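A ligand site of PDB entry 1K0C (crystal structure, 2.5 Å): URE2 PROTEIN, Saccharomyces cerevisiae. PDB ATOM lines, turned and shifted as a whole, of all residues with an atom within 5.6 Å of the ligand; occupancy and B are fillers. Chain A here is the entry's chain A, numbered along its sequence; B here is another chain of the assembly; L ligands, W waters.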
ATOM      1  N   SER A  27      -6.538 -34.864 -14.265  1.00  0.00           N
ATOM      2  CA  SER A  27      -5.105 -34.941 -14.004  1.00  0.00           C
ATOM      3  C   SER A  27      -4.629 -34.218 -12.747  1.00  0.00           C
ATOM      4  O   SER A  27      -3.431 -34.147 -12.487  1.00  0.00           O
ATOM      5  CB  SER A  27      -4.322 -34.397 -15.207  1.00  0.00           C
ATOM      6  OG  SER A  27      -4.432 -35.264 -16.321  1.00  0.00           O
ATOM      7  N   ALA A  28      -5.561 -33.691 -11.963  1.00  0.00           N
ATOM      8  CA  ALA A  28      -5.179 -32.949 -10.762  1.00  0.00           C
ATOM      9  C   ALA A  28      -5.024 -33.797  -9.508  1.00  0.00           C
ATOM     10  O   ALA A  28      -6.017 -34.219  -8.919  1.00  0.00           O
ATOM     11  CB  ALA A  28      -6.182 -31.829 -10.518  1.00  0.00           C
ATOM     12  N   PRO A  29      -3.779 -34.056  -9.074  1.00  0.00           N
ATOM     13  CA  PRO A  29      -3.638 -34.856  -7.859  1.00  0.00           C
ATOM     14  C   PRO A  29      -4.352 -34.134  -6.711  1.00  0.00           C
ATOM     15  O   PRO A  29      -4.926 -34.788  -5.841  1.00  0.00           O
ATOM     16  CB  PRO A  29      -2.117 -34.919  -7.665  1.00  0.00           C
ATOM     17  CG  PRO A  29      -1.598 -34.867  -9.080  1.00  0.00           C
ATOM     18  CD  PRO A  29      -2.474 -33.797  -9.699  1.00  0.00           C
ATOM     19  N   ASN A  30      -4.321 -32.801  -6.726  1.00  0.00           N
ATOM     20  CA  ASN A  30      -4.988 -31.979  -5.707  1.00  0.00           C
ATOM     21  C   ASN A  30      -6.469 -32.354  -5.569  1.00  0.00           C
ATOM     22  O   ASN A  30      -6.978 -32.502  -4.465  1.00  0.00           O
ATOM     23  CB  ASN A  30      -4.949 -30.495  -6.079  1.00  0.00           C
ATOM     24  CG  ASN A  30      -3.585 -29.906  -5.992  1.00  0.00           C
ATOM     25  OD1 ASN A  30      -2.935 -29.950  -4.934  1.00  0.00           O
ATOM     26  ND2 ASN A  30      -3.121 -29.340  -7.095  1.00  0.00           N
ATOM     27  N   LYS A  33      -7.073 -35.699  -4.047  1.00  0.00           N
ATOM     28  CA  LYS A  33      -6.737 -35.675  -2.640  1.00  0.00           C
ATOM     29  C   LYS A  33      -8.035 -35.370  -1.866  1.00  0.00           C
ATOM     30  O   LYS A  33      -8.332 -35.982  -0.839  1.00  0.00           O
ATOM     31  CB  LYS A  33      -5.679 -34.601  -2.368  1.00  0.00           C
ATOM     32  CG  LYS A  33      -5.183 -34.554  -0.933  1.00  0.00           C
ATOM     33  CD  LYS A  33      -4.055 -33.535  -0.770  1.00  0.00           C
ATOM     34  CE  LYS A  33      -4.533 -32.140  -1.107  1.00  0.00           C
ATOM     35  NZ  LYS A  33      -3.530 -31.096  -0.722  1.00  0.00           N
ATOM     36  N   PHE A  52     -10.214 -27.896 -19.448  1.00  0.00           N
ATOM     37  CA  PHE A  52      -9.529 -26.630 -19.589  1.00  0.00           C
ATOM     38  C   PHE A  52      -9.675 -26.119 -21.022  1.00  0.00           C
ATOM     39  O   PHE A  52      -9.540 -24.921 -21.280  1.00  0.00           O
ATOM     40  CB  PHE A  52      -8.042 -26.790 -19.206  1.00  0.00           C
ATOM     41  CG  PHE A  52      -7.830 -27.186 -17.761  1.00  0.00           C
ATOM     42  CD1 PHE A  52      -8.605 -26.644 -16.746  1.00  0.00           C
ATOM     43  CD2 PHE A  52      -6.828 -28.105 -17.419  1.00  0.00           C
ATOM     44  CE1 PHE A  52      -8.387 -26.984 -15.408  1.00  0.00           C
ATOM     45  CE2 PHE A  52      -6.599 -28.453 -16.084  1.00  0.00           C
ATOM     46  CZ  PHE A  52      -7.374 -27.893 -15.082  1.00  0.00           C
ATOM     47  N   HIS A  57     -12.627 -23.246 -16.254  1.00  0.00           N
ATOM     48  CA  HIS A  57     -12.007 -22.747 -15.029  1.00  0.00           C
ATOM     49  C   HIS A  57     -11.793 -21.235 -15.060  1.00  0.00           C
ATOM     50  O   HIS A  57     -11.436 -20.632 -14.051  1.00  0.00           O
ATOM     51  CB  HIS A  57     -10.680 -23.459 -14.767  1.00  0.00           C
ATOM     52  CG  HIS A  57      -9.629 -23.225 -15.820  1.00  0.00           C
ATOM     53  ND1 HIS A  57      -8.356 -23.746 -15.727  1.00  0.00           N
ATOM     54  CD2 HIS A  57      -9.655 -22.511 -16.964  1.00  0.00           C
ATOM     55  CE1 HIS A  57      -7.651 -23.373 -16.770  1.00  0.00           C
ATOM     56  NE2 HIS A  57      -8.418 -22.623 -17.544  1.00  0.00           N
ATOM     57  N   ARG A  58     -12.015 -20.638 -16.224  1.00  0.00           N
ATOM     58  CA  ARG A  58     -11.839 -19.199 -16.409  1.00  0.00           C
ATOM     59  C   ARG A  58     -13.205 -18.519 -16.361  1.00  0.00           C
ATOM     60  O   ARG A  58     -13.297 -17.308 -16.183  1.00  0.00           O
ATOM     61  CB  ARG A  58     -11.178 -18.924 -17.763  1.00  0.00           C
ATOM     62  CG  ARG A  58     -10.202 -17.754 -17.761  1.00  0.00           C
ATOM     63  CD  ARG A  58      -8.804 -18.206 -17.346  1.00  0.00           C
ATOM     64  NE  ARG A  58      -8.194 -19.074 -18.358  1.00  0.00           N
ATOM     65  CZ  ARG A  58      -7.021 -19.681 -18.222  1.00  0.00           C
ATOM     66  NH1 ARG A  58      -6.550 -20.446 -19.194  1.00  0.00           N
ATOM     67  NH2 ARG A  58      -6.319 -19.528 -17.098  1.00  0.00           N
ATOM     68  N   ASN A  68      -8.917 -17.844  -7.520  1.00  0.00           N
ATOM     69  CA  ASN A  68      -7.610 -18.238  -8.072  1.00  0.00           C
ATOM     70  C   ASN A  68      -7.768 -19.015  -9.390  1.00  0.00           C
ATOM     71  O   ASN A  68      -6.779 -19.374 -10.032  1.00  0.00           O
ATOM     72  CB  ASN A  68      -6.848 -19.097  -7.049  1.00  0.00           C
ATOM     73  CG  ASN A  68      -5.406 -19.341  -7.450  1.00  0.00           C
ATOM     74  OD1 ASN A  68      -4.876 -20.436  -7.272  1.00  0.00           O
ATOM     75  ND2 ASN A  68      -4.741 -18.312  -7.968  1.00  0.00           N
ATOM     76  N   ALA A  69      -9.024 -19.274  -9.779  1.00  0.00           N
ATOM     77  CA  ALA A  69      -9.334 -19.986 -11.018  1.00  0.00           C
ATOM     78  C   ALA A  69      -8.590 -21.306 -11.182  1.00  0.00           C
ATOM     79  O   ALA A  69      -8.101 -21.623 -12.274  1.00  0.00           O
ATOM     80  CB  ALA A  69      -9.064 -19.104 -12.220  1.00  0.00           C
ATOM     81  N   ARG A  70      -8.495 -22.071 -10.103  1.00  0.00           N
ATOM     82  CA  ARG A  70      -7.799 -23.353 -10.166  1.00  0.00           C
ATOM     83  C   ARG A  70      -8.610 -24.434  -9.457  1.00  0.00           C
ATOM     84  O   ARG A  70      -9.563 -24.141  -8.724  1.00  0.00           O
ATOM     85  CB  ARG A  70      -6.422 -23.245  -9.514  1.00  0.00           C
ATOM     86  CG  ARG A  70      -5.451 -22.283 -10.210  1.00  0.00           C
ATOM     87  CD  ARG A  70      -5.046 -22.778 -11.593  1.00  0.00           C
ATOM     88  NE  ARG A  70      -3.984 -21.985 -12.196  1.00  0.00           N
ATOM     89  CZ  ARG A  70      -4.158 -20.861 -12.889  1.00  0.00           C
ATOM     90  NH1 ARG A  70      -5.375 -20.365 -13.086  1.00  0.00           N
ATOM     91  NH2 ARG A  70      -3.103 -20.228 -13.384  1.00  0.00           N
ATOM     92  N   VAL A  71      -8.240 -25.680  -9.693  1.00  0.00           N
ATOM     93  CA  VAL A  71      -8.919 -26.797  -9.053  1.00  0.00           C
ATOM     94  C   VAL A  71      -7.968 -27.383  -8.014  1.00  0.00           C
ATOM     95  O   VAL A  71      -6.745 -27.319  -8.188  1.00  0.00           O
ATOM     96  CB  VAL A  71      -9.309 -27.903 -10.071  1.00  0.00           C
ATOM     97  CG1 VAL A  71     -10.242 -27.324 -11.120  1.00  0.00           C
ATOM     98  CG2 VAL A  71      -8.059 -28.502 -10.709  1.00  0.00           C
ATOM     99  N   PRO A  72      -8.519 -27.979  -6.951  1.00  0.00           N
ATOM    100  CA  PRO A  72      -9.955 -28.122  -6.736  1.00  0.00           C
ATOM    101  C   PRO A  72     -10.651 -27.006  -5.952  1.00  0.00           C
ATOM    102  O   PRO A  72     -10.015 -26.199  -5.266  1.00  0.00           O
ATOM    103  CB  PRO A  72     -10.057 -29.443  -5.997  1.00  0.00           C
ATOM    104  CG  PRO A  72      -8.897 -29.311  -5.045  1.00  0.00           C
ATOM    105  CD  PRO A  72      -7.777 -28.759  -5.939  1.00  0.00           C
ATOM    106  N   GLU A  86      -8.561 -24.208  -2.496  1.00  0.00           N
ATOM    107  CA  GLU A  86      -7.238 -24.610  -2.009  1.00  0.00           C
ATOM    108  C   GLU A  86      -7.437 -25.922  -1.255  1.00  0.00           C
ATOM    109  O   GLU A  86      -8.090 -25.971  -0.208  1.00  0.00           O
ATOM    110  CB  GLU A  86      -6.625 -23.554  -1.082  1.00  0.00           C
ATOM    111  CG  GLU A  86      -5.957 -22.431  -1.821  1.00  0.00           C
ATOM    112  CD  GLU A  86      -4.713 -22.877  -2.537  1.00  0.00           C
ATOM    113  OE1 GLU A  86      -4.393 -22.298  -3.588  1.00  0.00           O
ATOM    114  OE2 GLU A  86      -4.030 -23.788  -2.037  1.00  0.00           O
ATOM    115  N   SER A  87      -6.881 -26.997  -1.816  1.00  0.00           N
ATOM    116  CA  SER A  87      -6.984 -28.333  -1.244  1.00  0.00           C
ATOM    117  C   SER A  87      -6.648 -28.414   0.254  1.00  0.00           C
ATOM    118  O   SER A  87      -7.272 -29.182   0.996  1.00  0.00           O
ATOM    119  CB  SER A  87      -6.114 -29.316  -2.031  1.00  0.00           C
ATOM    120  OG  SER A  87      -4.753 -28.933  -2.001  1.00  0.00           O
ATOM    121  N   GLY A  88      -5.650 -27.641   0.692  1.00  0.00           N
ATOM    122  CA  GLY A  88      -5.284 -27.650   2.098  1.00  0.00           C
ATOM    123  C   GLY A  88      -6.436 -27.166   2.963  1.00  0.00           C
ATOM    124  O   GLY A  88      -6.796 -27.793   3.964  1.00  0.00           O
ATOM    125  N   THR A 126       1.490 -29.253   0.589  1.00  0.00           N
ATOM    126  CA  THR A 126       0.945 -28.254  -0.345  1.00  0.00           C
ATOM    127  C   THR A 126       1.879 -27.117  -0.734  1.00  0.00           C
ATOM    128  O   THR A 126       1.708 -26.530  -1.799  1.00  0.00           O
ATOM    129  CB  THR A 126      -0.350 -27.607   0.192  1.00  0.00           C
ATOM    130  OG1 THR A 126      -0.087 -26.981   1.443  1.00  0.00           O
ATOM    131  CG2 THR A 126      -1.448 -28.657   0.354  1.00  0.00           C
ATOM    132  N   ILE A 133       6.877 -30.605  -7.634  1.00  0.00           N
ATOM    133  CA  ILE A 133       6.580 -31.658  -8.588  1.00  0.00           C
ATOM    134  C   ILE A 133       6.065 -30.960  -9.851  1.00  0.00           C
ATOM    135  O   ILE A 133       6.541 -31.210 -10.964  1.00  0.00           O
ATOM    136  CB  ILE A 133       5.495 -32.609  -8.044  1.00  0.00           C
ATOM    137  CG1 ILE A 133       6.078 -33.447  -6.902  1.00  0.00           C
ATOM    138  CG2 ILE A 133       4.973 -33.506  -9.150  1.00  0.00           C
ATOM    139  CD1 ILE A 133       5.024 -34.185  -6.061  1.00  0.00           C
ATOM    140  N   GLY A 134       5.115 -30.046  -9.664  1.00  0.00           N
ATOM    141  CA  GLY A 134       4.557 -29.301 -10.775  1.00  0.00           C
ATOM    142  C   GLY A 134       5.594 -28.560 -11.618  1.00  0.00           C
ATOM    143  O   GLY A 134       5.485 -28.535 -12.847  1.00  0.00           O
ATOM    144  N   LEU A 137       7.574 -31.075 -13.605  1.00  0.00           N
ATOM    145  CA  LEU A 137       6.834 -31.546 -14.764  1.00  0.00           C
ATOM    146  C   LEU A 137       6.912 -30.526 -15.892  1.00  0.00           C
ATOM    147  O   LEU A 137       7.169 -30.876 -17.047  1.00  0.00           O
ATOM    148  CB  LEU A 137       5.364 -31.784 -14.420  1.00  0.00           C
ATOM    149  CG  LEU A 137       5.060 -33.067 -13.645  1.00  0.00           C
ATOM    150  CD1 LEU A 137       3.653 -33.006 -13.063  1.00  0.00           C
ATOM    151  CD2 LEU A 137       5.234 -34.260 -14.577  1.00  0.00           C
ATOM    152  N   TRP A 222       0.024 -37.542  -5.277  1.00  0.00           N
ATOM    153  CA  TRP A 222       1.294 -37.063  -5.825  1.00  0.00           C
ATOM    154  C   TRP A 222       2.348 -38.158  -5.906  1.00  0.00           C
ATOM    155  O   TRP A 222       3.230 -38.118  -6.779  1.00  0.00           O
ATOM    156  CB  TRP A 222       1.801 -35.890  -4.984  1.00  0.00           C
ATOM    157  CG  TRP A 222       0.841 -34.748  -4.987  1.00  0.00           C
ATOM    158  CD1 TRP A 222      -0.129 -34.483  -4.054  1.00  0.00           C
ATOM    159  CD2 TRP A 222       0.711 -33.745  -6.002  1.00  0.00           C
ATOM    160  NE1 TRP A 222      -0.858 -33.376  -4.433  1.00  0.00           N
ATOM    161  CE2 TRP A 222      -0.366 -32.909  -5.622  1.00  0.00           C
ATOM    162  CE3 TRP A 222       1.393 -33.480  -7.186  1.00  0.00           C
ATOM    163  CZ2 TRP A 222      -0.764 -31.823  -6.399  1.00  0.00           C
ATOM    164  CZ3 TRP A 222       0.990 -32.399  -7.970  1.00  0.00           C
ATOM    165  CH2 TRP A 222      -0.085 -31.586  -7.560  1.00  0.00           C
ATOM    166  N   VAL A 225       2.426 -39.963  -9.048  1.00  0.00           N
ATOM    167  CA  VAL A 225       2.755 -39.108 -10.174  1.00  0.00           C
ATOM    168  C   VAL A 225       4.250 -38.857 -10.385  1.00  0.00           C
ATOM    169  O   VAL A 225       4.683 -38.553 -11.508  1.00  0.00           O
ATOM    170  CB  VAL A 225       1.981 -37.754 -10.039  1.00  0.00           C
ATOM    171  CG1 VAL A 225       2.829 -36.580 -10.473  1.00  0.00           C
ATOM    172  CG2 VAL A 225       0.692 -37.820 -10.841  1.00  0.00           C
ATOM    173  N   ARG A 228       6.635 -39.933 -13.315  1.00  0.00           N
ATOM    174  CA  ARG A 228       6.694 -39.169 -14.554  1.00  0.00           C
ATOM    175  C   ARG A 228       7.893 -38.207 -14.602  1.00  0.00           C
ATOM    176  O   ARG A 228       8.140 -37.568 -15.621  1.00  0.00           O
ATOM    177  CB  ARG A 228       5.376 -38.407 -14.785  1.00  0.00           C
ATOM    178  CG  ARG A 228       4.152 -39.238 -14.437  1.00  0.00           C
ATOM    179  CD  ARG A 228       2.928 -38.977 -15.308  1.00  0.00           C
ATOM    180  NE  ARG A 228       2.483 -37.581 -15.330  1.00  0.00           N
ATOM    181  CZ  ARG A 228       2.916 -36.680 -16.203  1.00  0.00           C
ATOM    182  NH1 ARG A 228       3.811 -37.002 -17.136  1.00  0.00           N
ATOM    183  NH2 ARG A 228       2.432 -35.442 -16.167  1.00  0.00           N
ATOM    184  N   PHE B 123      -3.471 -20.922   2.682  1.00  0.00           N
ATOM    185  CA  PHE B 123      -2.819 -21.938   1.847  1.00  0.00           C
ATOM    186  C   PHE B 123      -2.438 -21.326   0.496  1.00  0.00           C
ATOM    187  O   PHE B 123      -1.388 -21.644  -0.076  1.00  0.00           O
ATOM    188  CB  PHE B 123      -3.742 -23.158   1.644  1.00  0.00           C
ATOM    189  CG  PHE B 123      -3.594 -24.201   2.719  1.00  0.00           C
ATOM    190  CD1 PHE B 123      -4.450 -24.229   3.815  1.00  0.00           C
ATOM    191  CD2 PHE B 123      -2.570 -25.141   2.654  1.00  0.00           C
ATOM    192  CE1 PHE B 123      -4.289 -25.161   4.828  1.00  0.00           C
ATOM    193  CE2 PHE B 123      -2.395 -26.087   3.679  1.00  0.00           C
ATOM    194  CZ  PHE B 123      -3.263 -26.089   4.767  1.00  0.00           C
ATOM    195  N   SER B 127       1.163 -21.670  -0.594  1.00  0.00           N
ATOM    196  CA  SER B 127       1.317 -22.574  -1.721  1.00  0.00           C
ATOM    197  C   SER B 127       1.524 -21.902  -3.076  1.00  0.00           C
ATOM    198  O   SER B 127       2.326 -22.379  -3.877  1.00  0.00           O
ATOM    199  CB  SER B 127       0.109 -23.499  -1.812  1.00  0.00           C
ATOM    200  OG  SER B 127      -0.100 -24.134  -0.573  1.00  0.00           O
ATOM    201  N   GLY B 128       0.817 -20.809  -3.329  1.00  0.00           N
ATOM    202  CA  GLY B 128       0.932 -20.155  -4.623  1.00  0.00           C
ATOM    203  C   GLY B 128       1.622 -18.809  -4.676  1.00  0.00           C
ATOM    204  O   GLY B 128       2.067 -18.376  -5.741  1.00  0.00           O
HETATM  205  N1  LIG L   1      -2.380 -24.730  -4.046  1.00  0.00           N
HETATM  206  C1  LIG L   1      -3.477 -25.109  -4.930  1.00  0.00           C
HETATM  207  C2  LIG L   1      -4.109 -26.296  -4.129  1.00  0.00           C
HETATM  208  O1  LIG L   1      -3.375 -26.955  -3.378  1.00  0.00           O
HETATM  209  O2  LIG L   1      -5.326 -26.534  -4.251  1.00  0.00           O
HETATM  210  C3  LIG L   1      -2.925 -25.517  -6.320  1.00  0.00           C
HETATM  211  C4  LIG L   1      -4.024 -25.944  -7.301  1.00  0.00           C
HETATM  212  C5  LIG L   1      -3.452 -26.311  -8.664  1.00  0.00           C
HETATM  213  O3  LIG L   1      -2.228 -26.250  -8.911  1.00  0.00           O
HETATM  214  N2  LIG L   1      -4.381 -26.683  -9.543  1.00  0.00           N
HETATM  215  C6  LIG L   1      -4.024 -27.051 -10.934  1.00  0.00           C
HETATM  216  C7  LIG L   1      -4.948 -26.281 -11.876  1.00  0.00           C
HETATM  217  O4  LIG L   1      -6.078 -25.939 -11.524  1.00  0.00           O
HETATM  218  C8  LIG L   1      -4.220 -28.556 -11.223  1.00  0.00           C
HETATM  219  S1  LIG L   1      -3.170 -29.665 -10.258  1.00  0.00           S
HETATM  220  N3  LIG L   1      -4.443 -26.019 -13.075  1.00  0.00           N
HETATM  221  C9  LIG L   1      -5.183 -25.297 -14.091  1.00  0.00           C
HETATM  222  C10 LIG L   1      -4.297 -25.130 -15.286  1.00  0.00           C
HETATM  223  O5  LIG L   1      -3.861 -26.158 -15.825  1.00  0.00           O
HETATM  224  O6  LIG L   1      -4.049 -23.959 -15.663  1.00  0.00           O
HETATM  225  C11 LIG L   1      -1.668 -29.403 -11.275  1.00  0.00           C
HETATM  226  C12 LIG L   1      -1.154 -30.715 -11.867  1.00  0.00           C
HETATM  227  C13 LIG L   1      -0.187 -31.463 -11.171  1.00  0.00           C
HETATM  228  C14 LIG L   1       0.283 -32.677 -11.693  1.00  0.00           C
HETATM  229  C15 LIG L   1      -0.205 -33.194 -12.940  1.00  0.00           C
HETATM  230  N4  LIG L   1       0.330 -34.519 -13.465  1.00  0.00           N
HETATM  231  O7  LIG L   1       1.167 -35.166 -12.839  1.00  0.00           O
HETATM  232  O8  LIG L   1      -0.087 -34.970 -14.521  1.00  0.00           O
HETATM  233  C16 LIG L   1      -1.189 -32.460 -13.686  1.00  0.00           C
HETATM  234  C17 LIG L   1      -1.694 -31.240 -13.199  1.00  0.00           C
HETATM  235  O   HOH W   1      -2.073 -21.736  -4.777  1.00  0.00           O
HETATM  236  O   HOH W   2      -0.572 -26.756  -3.389  1.00  0.00           O
HETATM  237  O   HOH W   3      -7.534 -25.114  -5.268  1.00  0.00           O
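OE2 of Glu 86 is in salt-bridge range of N1 of the ligand (2.8 Å).
The backbone NH (N) of Ser 87 lies within hydrogen-bond range of an oxygen (O2) of the ligand, at 2.9 Å.
The side-chain hydroxyl (OG) of Ser 87 is in hydrogen-bond range of an oxygen (O1) of the ligand (2.8 Å).
An oxygen (O4) of the ligand lies within hydrogen-bond range of the backbone NH (N) of Val 71 (2.8 Å).
A nitrogen (N2) of the ligand sits at hydrogen-bond distance from the backbone carbonyl oxygen of Val 71.
An oxygen (O8) of the ligand lies within hydrogen-bond range of the guanidinium group of Arg 228 (3.0 Å).
The side-chain amide nitrogen (ND2) of Asn 30 sits close to a sulfur (S1) of the ligand, at 3.2 Å.
The guanidinium group (NE) of Arg 70 lies within salt-bridge range of an oxygen (O6) of the ligand (3.99 Å).
NZ of Lys 33 is in hydrogen-bond range of OG of Ser 87, at 2.8 Å.
The side-chain hydroxyl (OG) of Ser 127 of chain B is in hydrogen-bond range of the backbone carbonyl oxygen (O) of Thr 126, at 3.2 Å.
O of Phe 123 of chain B is in hydrogen-bond range of OG of Ser 127 of chain B, at 2.8 Å.
NE2 of His 57 lies within hydrogen-bond range of NH1 of Arg 58 (3.3 Å).
Residues that only touch the ligand: Ser 27, Ala 28, Pro 29, Phe 52, His 57, Pro 72, Leu 137, Trp 222, Val 225 and Ser 127 of chain B.
16 residues have an atom within 4 Å of the ligand: Ser 27, Ala 28, Pro 29, Asn 30, Phe 52, His 57, Arg 70, Val 71, Pro 72, Glu 86, Ser 87, Leu 137, Trp 222, Val 225, Arg 228 and Ser 127 of chain B.
The nearest printed residue that does not touch the ligand is Thr 126 (4.5 Å).
Water W2 lies within hydrogen-bond range of O of Thr 126 and N1 of the ligand.
Water W3 lies within hydrogen-bond range of O of Pro 72 (2.7 Å), O2 of the ligand (2.8 Å) and N of Glu 86 (3.1 Å).
Water W1 lies within hydrogen-bond range of OE1 of Glu 86 (2.7 Å), N1 of the ligand (3.1 Å) and N of Gly 128 of chain B (3.4 Å).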
